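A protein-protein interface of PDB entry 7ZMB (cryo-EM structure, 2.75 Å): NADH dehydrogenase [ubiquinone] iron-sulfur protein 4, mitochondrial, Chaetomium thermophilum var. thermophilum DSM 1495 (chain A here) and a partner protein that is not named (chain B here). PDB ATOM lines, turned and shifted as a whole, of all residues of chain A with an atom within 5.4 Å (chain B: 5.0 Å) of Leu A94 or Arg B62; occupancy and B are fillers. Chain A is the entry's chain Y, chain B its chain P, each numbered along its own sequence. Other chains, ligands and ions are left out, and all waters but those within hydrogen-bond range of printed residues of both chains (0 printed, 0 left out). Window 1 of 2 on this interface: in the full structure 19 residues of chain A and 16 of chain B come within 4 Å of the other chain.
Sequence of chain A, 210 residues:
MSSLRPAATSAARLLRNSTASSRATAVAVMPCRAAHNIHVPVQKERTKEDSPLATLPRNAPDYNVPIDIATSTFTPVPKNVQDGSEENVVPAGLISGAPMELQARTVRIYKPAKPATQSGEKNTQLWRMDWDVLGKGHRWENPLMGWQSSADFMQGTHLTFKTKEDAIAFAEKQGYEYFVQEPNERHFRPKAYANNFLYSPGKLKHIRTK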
ATOM      1  N   PRO A  66     -17.693 -28.135  -5.775  1.00  0.00           N
ATOM      2  CA  PRO A  66     -18.306 -29.466  -5.834  1.00  0.00           C
ATOM      3  C   PRO A  66     -19.090 -29.669  -7.120  1.00  0.00           C
ATOM      4  O   PRO A  66     -19.630 -28.728  -7.706  1.00  0.00           O
ATOM      5  CB  PRO A  66     -19.227 -29.486  -4.611  1.00  0.00           C
ATOM      6  CG  PRO A  66     -19.526 -28.049  -4.344  1.00  0.00           C
ATOM      7  CD  PRO A  66     -18.286 -27.295  -4.722  1.00  0.00           C
ATOM      8  N   GLN A  82     -22.731 -18.625  -6.059  1.00  0.00           N
ATOM      9  CA  GLN A  82     -23.439 -17.964  -4.975  1.00  0.00           C
ATOM     10  C   GLN A  82     -23.488 -18.866  -3.750  1.00  0.00           C
ATOM     11  O   GLN A  82     -23.525 -20.092  -3.853  1.00  0.00           O
ATOM     12  CB  GLN A  82     -24.862 -17.597  -5.398  1.00  0.00           C
ATOM     13  CG  GLN A  82     -25.001 -16.321  -6.212  1.00  0.00           C
ATOM     14  CD  GLN A  82     -26.390 -16.180  -6.805  1.00  0.00           C
ATOM     15  OE1 GLN A  82     -27.106 -17.166  -6.959  1.00  0.00           O
ATOM     16  NE2 GLN A  82     -26.776 -14.961  -7.141  1.00  0.00           N
ATOM     17  N   ASP A  83     -23.491 -18.245  -2.575  1.00  0.00           N
ATOM     18  CA  ASP A  83     -23.701 -18.968  -1.331  1.00  0.00           C
ATOM     19  C   ASP A  83     -24.731 -18.306  -0.430  1.00  0.00           C
ATOM     20  O   ASP A  83     -25.022 -18.842   0.642  1.00  0.00           O
ATOM     21  CB  ASP A  83     -22.382 -19.126  -0.565  1.00  0.00           C
ATOM     22  CG  ASP A  83     -21.900 -17.832   0.041  1.00  0.00           C
ATOM     23  OD1 ASP A  83     -22.271 -16.756  -0.469  1.00  0.00           O
ATOM     24  OD2 ASP A  83     -21.146 -17.888   1.032  1.00  0.00           O
ATOM     25  N   GLY A  84     -25.289 -17.173  -0.831  1.00  0.00           N
ATOM     26  CA  GLY A  84     -26.292 -16.510  -0.034  1.00  0.00           C
ATOM     27  C   GLY A  84     -25.777 -15.495   0.959  1.00  0.00           C
ATOM     28  O   GLY A  84     -26.577 -14.952   1.727  1.00  0.00           O
ATOM     29  N   PRO A  91     -29.979 -14.645  -3.821  1.00  0.00           N
ATOM     30  CA  PRO A  91     -29.209 -15.751  -4.416  1.00  0.00           C
ATOM     31  C   PRO A  91     -30.139 -16.789  -5.029  1.00  0.00           C
ATOM     32  O   PRO A  91     -30.351 -17.888  -4.513  1.00  0.00           O
ATOM     33  CB  PRO A  91     -28.426 -16.281  -3.213  1.00  0.00           C
ATOM     34  CG  PRO A  91     -29.343 -16.076  -2.084  1.00  0.00           C
ATOM     35  CD  PRO A  91     -30.157 -14.832  -2.372  1.00  0.00           C
ATOM     36  N   ALA A  92     -30.738 -16.422  -6.159  1.00  0.00           N
ATOM     37  CA  ALA A  92     -31.705 -17.308  -6.793  1.00  0.00           C
ATOM     38  C   ALA A  92     -31.033 -18.552  -7.346  1.00  0.00           C
ATOM     39  O   ALA A  92     -31.567 -19.655  -7.212  1.00  0.00           O
ATOM     40  CB  ALA A  92     -32.467 -16.562  -7.888  1.00  0.00           C
ATOM     41  N   GLY A  93     -29.857 -18.398  -7.956  1.00  0.00           N
ATOM     42  CA  GLY A  93     -29.145 -19.536  -8.501  1.00  0.00           C
ATOM     43  C   GLY A  93     -28.716 -20.550  -7.462  1.00  0.00           C
ATOM     44  O   GLY A  93     -28.455 -21.705  -7.805  1.00  0.00           O
ATOM     45  N   LEU A  94     -28.626 -20.141  -6.198  1.00  0.00           N
ATOM     46  CA  LEU A  94     -28.320 -21.089  -5.138  1.00  0.00           C
ATOM     47  C   LEU A  94     -29.517 -21.976  -4.821  1.00  0.00           C
ATOM     48  O   LEU A  94     -29.354 -23.163  -4.518  1.00  0.00           O
ATOM     49  CB  LEU A  94     -27.857 -20.336  -3.893  1.00  0.00           C
ATOM     50  CG  LEU A  94     -27.687 -21.136  -2.613  1.00  0.00           C
ATOM     51  CD1 LEU A  94     -26.493 -22.029  -2.727  1.00  0.00           C
ATOM     52  CD2 LEU A  94     -27.549 -20.184  -1.453  1.00  0.00           C
ATOM     53  N   ILE A  95     -30.727 -21.428  -4.906  1.00  0.00           N
ATOM     54  CA  ILE A  95     -31.946 -22.143  -4.547  1.00  0.00           C
ATOM     55  C   ILE A  95     -32.790 -22.513  -5.753  1.00  0.00           C
ATOM     56  O   ILE A  95     -33.879 -23.076  -5.574  1.00  0.00           O
ATOM     57  CB  ILE A  95     -32.791 -21.335  -3.543  1.00  0.00           C
ATOM     58  CG1 ILE A  95     -32.951 -19.895  -4.023  1.00  0.00           C
ATOM     59  CG2 ILE A  95     -32.168 -21.374  -2.161  1.00  0.00           C
ATOM     60  CD1 ILE A  95     -34.050 -19.138  -3.351  1.00  0.00           C
ATOM     61  N   SER A  96     -32.336 -22.215  -6.972  1.00  0.00           N
ATOM     62  CA  SER A  96     -33.170 -22.448  -8.148  1.00  0.00           C
ATOM     63  C   SER A  96     -33.245 -23.915  -8.525  1.00  0.00           C
ATOM     64  O   SER A  96     -34.273 -24.366  -9.039  1.00  0.00           O
ATOM     65  CB  SER A  96     -32.657 -21.647  -9.345  1.00  0.00           C
ATOM     66  OG  SER A  96     -31.500 -22.233  -9.892  1.00  0.00           O
ATOM     67  N   GLY A  97     -32.189 -24.669  -8.284  1.00  0.00           N
ATOM     68  CA  GLY A  97     -32.113 -26.027  -8.744  1.00  0.00           C
ATOM     69  C   GLY A  97     -31.313 -26.214 -10.007  1.00  0.00           C
ATOM     70  O   GLY A  97     -31.033 -27.356 -10.378  1.00  0.00           O
ATOM     71  N   MET A 100     -24.461 -25.992 -11.190  1.00  0.00           N
ATOM     72  CA  MET A 100     -23.434 -24.980 -10.988  1.00  0.00           C
ATOM     73  C   MET A 100     -22.846 -24.494 -12.300  1.00  0.00           C
ATOM     74  O   MET A 100     -22.199 -23.443 -12.325  1.00  0.00           O
ATOM     75  CB  MET A 100     -22.316 -25.527 -10.104  1.00  0.00           C
ATOM     76  CG  MET A 100     -22.752 -25.847  -8.696  1.00  0.00           C
ATOM     77  SD  MET A 100     -23.360 -24.419  -7.782  1.00  0.00           S
ATOM     78  CE  MET A 100     -25.132 -24.683  -7.875  1.00  0.00           C
ATOM     79  N   GLN A 103     -23.366 -20.883 -13.343  1.00  0.00           N
ATOM     80  CA  GLN A 103     -22.580 -19.831 -12.728  1.00  0.00           C
ATOM     81  C   GLN A 103     -21.141 -19.850 -13.202  1.00  0.00           C
ATOM     82  O   GLN A 103     -20.368 -18.965 -12.833  1.00  0.00           O
ATOM     83  CB  GLN A 103     -22.666 -19.959 -11.207  1.00  0.00           C
ATOM     84  CG  GLN A 103     -24.095 -20.171 -10.745  1.00  0.00           C
ATOM     85  CD  GLN A 103     -24.284 -19.984  -9.266  1.00  0.00           C
ATOM     86  OE1 GLN A 103     -23.878 -18.976  -8.698  1.00  0.00           O
ATOM     87  NE2 GLN A 103     -24.919 -20.952  -8.630  1.00  0.00           N
ATOM     88  N   GLN B  58     -22.974 -32.470   4.503  1.00  0.00           N
ATOM     89  CA  GLN B  58     -22.483 -31.638   3.409  1.00  0.00           C
ATOM     90  C   GLN B  58     -23.602 -30.853   2.747  1.00  0.00           C
ATOM     91  O   GLN B  58     -23.384 -29.722   2.301  1.00  0.00           O
ATOM     92  CB  GLN B  58     -21.775 -32.499   2.368  1.00  0.00           C
ATOM     93  CG  GLN B  58     -20.690 -33.388   2.925  1.00  0.00           C
ATOM     94  CD  GLN B  58     -20.362 -34.522   1.998  1.00  0.00           C
ATOM     95  OE1 GLN B  58     -21.242 -35.059   1.328  1.00  0.00           O
ATOM     96  NE2 GLN B  58     -19.089 -34.895   1.942  1.00  0.00           N
ATOM     97  N   GLU B  59     -24.793 -31.443   2.647  1.00  0.00           N
ATOM     98  CA  GLU B  59     -25.927 -30.716   2.094  1.00  0.00           C
ATOM     99  C   GLU B  59     -26.279 -29.524   2.962  1.00  0.00           C
ATOM    100  O   GLU B  59     -26.593 -28.447   2.449  1.00  0.00           O
ATOM    101  CB  GLU B  59     -27.134 -31.641   1.946  1.00  0.00           C
ATOM    102  CG  GLU B  59     -27.112 -32.483   0.690  1.00  0.00           C
ATOM    103  CD  GLU B  59     -27.022 -31.646  -0.577  1.00  0.00           C
ATOM    104  OE1 GLU B  59     -27.651 -30.568  -0.634  1.00  0.00           O
ATOM    105  OE2 GLU B  59     -26.315 -32.067  -1.517  1.00  0.00           O
ATOM    106  N   PHE B  60     -26.237 -29.702   4.283  1.00  0.00           N
ATOM    107  CA  PHE B  60     -26.484 -28.586   5.184  1.00  0.00           C
ATOM    108  C   PHE B  60     -25.353 -27.572   5.141  1.00  0.00           C
ATOM    109  O   PHE B  60     -25.597 -26.375   5.297  1.00  0.00           O
ATOM    110  CB  PHE B  60     -26.694 -29.092   6.610  1.00  0.00           C
ATOM    111  CG  PHE B  60     -28.133 -29.282   6.973  1.00  0.00           C
ATOM    112  CD1 PHE B  60     -28.910 -28.205   7.350  1.00  0.00           C
ATOM    113  CD2 PHE B  60     -28.715 -30.530   6.928  1.00  0.00           C
ATOM    114  CE1 PHE B  60     -30.227 -28.373   7.676  1.00  0.00           C
ATOM    115  CE2 PHE B  60     -30.036 -30.703   7.251  1.00  0.00           C
ATOM    116  CZ  PHE B  60     -30.793 -29.625   7.621  1.00  0.00           C
ATOM    117  N   GLU B  61     -24.121 -28.029   4.920  1.00  0.00           N
ATOM    118  CA  GLU B  61     -22.973 -27.129   4.935  1.00  0.00           C
ATOM    119  C   GLU B  61     -22.950 -26.198   3.728  1.00  0.00           C
ATOM    120  O   GLU B  61     -22.356 -25.119   3.801  1.00  0.00           O
ATOM    121  CB  GLU B  61     -21.675 -27.935   5.002  1.00  0.00           C
ATOM    122  CG  GLU B  61     -21.334 -28.468   6.382  1.00  0.00           C
ATOM    123  CD  GLU B  61     -20.663 -27.436   7.279  1.00  0.00           C
ATOM    124  OE1 GLU B  61     -21.157 -26.292   7.367  1.00  0.00           O
ATOM    125  OE2 GLU B  61     -19.635 -27.777   7.903  1.00  0.00           O
ATOM    126  N   ARG B  62     -23.553 -26.596   2.607  1.00  0.00           N
ATOM    127  CA  ARG B  62     -23.533 -25.730   1.436  1.00  0.00           C
ATOM    128  C   ARG B  62     -24.402 -24.490   1.625  1.00  0.00           C
ATOM    129  O   ARG B  62     -24.172 -23.479   0.957  1.00  0.00           O
ATOM    130  CB  ARG B  62     -23.952 -26.530   0.198  1.00  0.00           C
ATOM    131  CG  ARG B  62     -23.993 -25.750  -1.113  1.00  0.00           C
ATOM    132  CD  ARG B  62     -24.141 -26.697  -2.311  1.00  0.00           C
ATOM    133  NE  ARG B  62     -25.403 -27.432  -2.342  1.00  0.00           N
ATOM    134  CZ  ARG B  62     -26.583 -26.883  -2.609  1.00  0.00           C
ATOM    135  NH1 ARG B  62     -27.678 -27.631  -2.610  1.00  0.00           N
ATOM    136  NH2 ARG B  62     -26.667 -25.594  -2.913  1.00  0.00           N
ATOM    137  N   HIS B  63     -25.317 -24.525   2.599  1.00  0.00           N
ATOM    138  CA  HIS B  63     -26.198 -23.362   2.883  1.00  0.00           C
ATOM    139  C   HIS B  63     -25.733 -22.703   4.180  1.00  0.00           C
ATOM    140  O   HIS B  63     -26.461 -21.828   4.674  1.00  0.00           O
ATOM    141  CB  HIS B  63     -27.667 -23.794   2.872  1.00  0.00           C
ATOM    142  CG  HIS B  63     -28.043 -24.542   1.640  1.00  0.00           C
ATOM    143  ND1 HIS B  63     -28.396 -25.876   1.667  1.00  0.00           N
ATOM    144  CD2 HIS B  63     -28.093 -24.161   0.347  1.00  0.00           C
ATOM    145  CE1 HIS B  63     -28.666 -26.280   0.443  1.00  0.00           C
ATOM    146  NE2 HIS B  63     -28.488 -25.245  -0.384  1.00  0.00           N
ATOM    147  N   ARG B  64     -24.555 -23.082   4.676  1.00  0.00           N
ATOM    148  CA  ARG B  64     -23.988 -22.547   5.911  1.00  0.00           C
ATOM    149  C   ARG B  64     -24.032 -21.021   5.959  1.00  0.00           C
ATOM    150  O   ARG B  64     -24.536 -20.449   6.927  1.00  0.00           O
ATOM    151  CB  ARG B  64     -22.545 -23.044   5.996  1.00  0.00           C
ATOM    152  CG  ARG B  64     -21.669 -22.684   7.179  1.00  0.00           C
ATOM    153  CD  ARG B  64     -22.073 -23.269   8.504  1.00  0.00           C
ATOM    154  NE  ARG B  64     -21.091 -22.865   9.505  1.00  0.00           N
ATOM    155  CZ  ARG B  64     -21.212 -23.066  10.810  1.00  0.00           C
ATOM    156  NH1 ARG B  64     -22.271 -23.690  11.288  1.00  0.00           N
ATOM    157  NH2 ARG B  64     -20.257 -22.660  11.634  1.00  0.00           N
ATOM    158  N   VAL B  66     -25.654 -18.360   4.790  1.00  0.00           N
ATOM    159  CA  VAL B  66     -26.829 -17.640   4.321  1.00  0.00           C
ATOM    160  C   VAL B  66     -27.302 -16.727   5.443  1.00  0.00           C
ATOM    161  O   VAL B  66     -27.511 -17.176   6.575  1.00  0.00           O
ATOM    162  CB  VAL B  66     -27.942 -18.603   3.871  1.00  0.00           C
ATOM    163  CG1 VAL B  66     -29.240 -17.868   3.684  1.00  0.00           C
ATOM    164  CG2 VAL B  66     -27.567 -19.256   2.570  1.00  0.00           C
ATOM    165  N   VAL B  71     -34.424 -16.747   2.323  1.00  0.00           N
ATOM    166  CA  VAL B  71     -33.756 -17.821   1.604  1.00  0.00           C
ATOM    167  C   VAL B  71     -33.685 -19.081   2.459  1.00  0.00           C
ATOM    168  O   VAL B  71     -33.852 -20.190   1.947  1.00  0.00           O
ATOM    169  CB  VAL B  71     -32.361 -17.369   1.125  1.00  0.00           C
ATOM    170  CG1 VAL B  71     -31.627 -18.505   0.437  1.00  0.00           C
ATOM    171  CG2 VAL B  71     -32.488 -16.207   0.186  1.00  0.00           C
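A ring nitrogen (NE2) of His B63 is in hydrogen-bond range of the guanidinium group of Arg B62 (3.1 Å). The backbone NH (N) of Leu A94 lies within hydrogen-bond range of the side-chain amide oxygen (OE1) of Gln A82. The side-chain carboxylate (OE1) of Glu B59 is in salt-bridge range of the guanidinium group (NH1) of Arg B62.
Of chain B, only Arg B62 comes within 4 Å of Leu A94. Arg B62 touches one residue of chain A. Printed residues of chain A within 4 Å of Val B66: Asp A83 and Gly A84. Printed residues of chain B within 4 Å of Ile A95: Val B71 (3.9 Å). Arg B64 touches none of the printed residues of chain A. The nearest printed residue of chain A that does not touch Val B71 is Leu A94 (4.8 Å).
Among the printed residues, merely in contact across the chains: Asp A83 with Val B66 (3.2 Å), Leu A94 with Arg B62 (3.6 Å), Pro A91 with Val B71 (3.7 Å), Gly A84 with Val B66 (3.7 Å) and Ile A95 with Val B71 (3.9 Å).
Along chain B the printed residues that touch a printed residue of chain A span positions 62 to 71. Of the 13 printed residues of chain A, 5 touch a printed residue of chain B. Hydrophobic or aromatic side chains of chain A that line the printed part of chain B: Pro A91, Leu A94 and Ile A95. Along chain A the printed residues that touch a printed residue of chain B span positions 83 to 95. Among the printed residues, no Asp or Glu carboxylate lies within 4 Å of a Lys or Arg side-chain nitrogen of the other chain.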
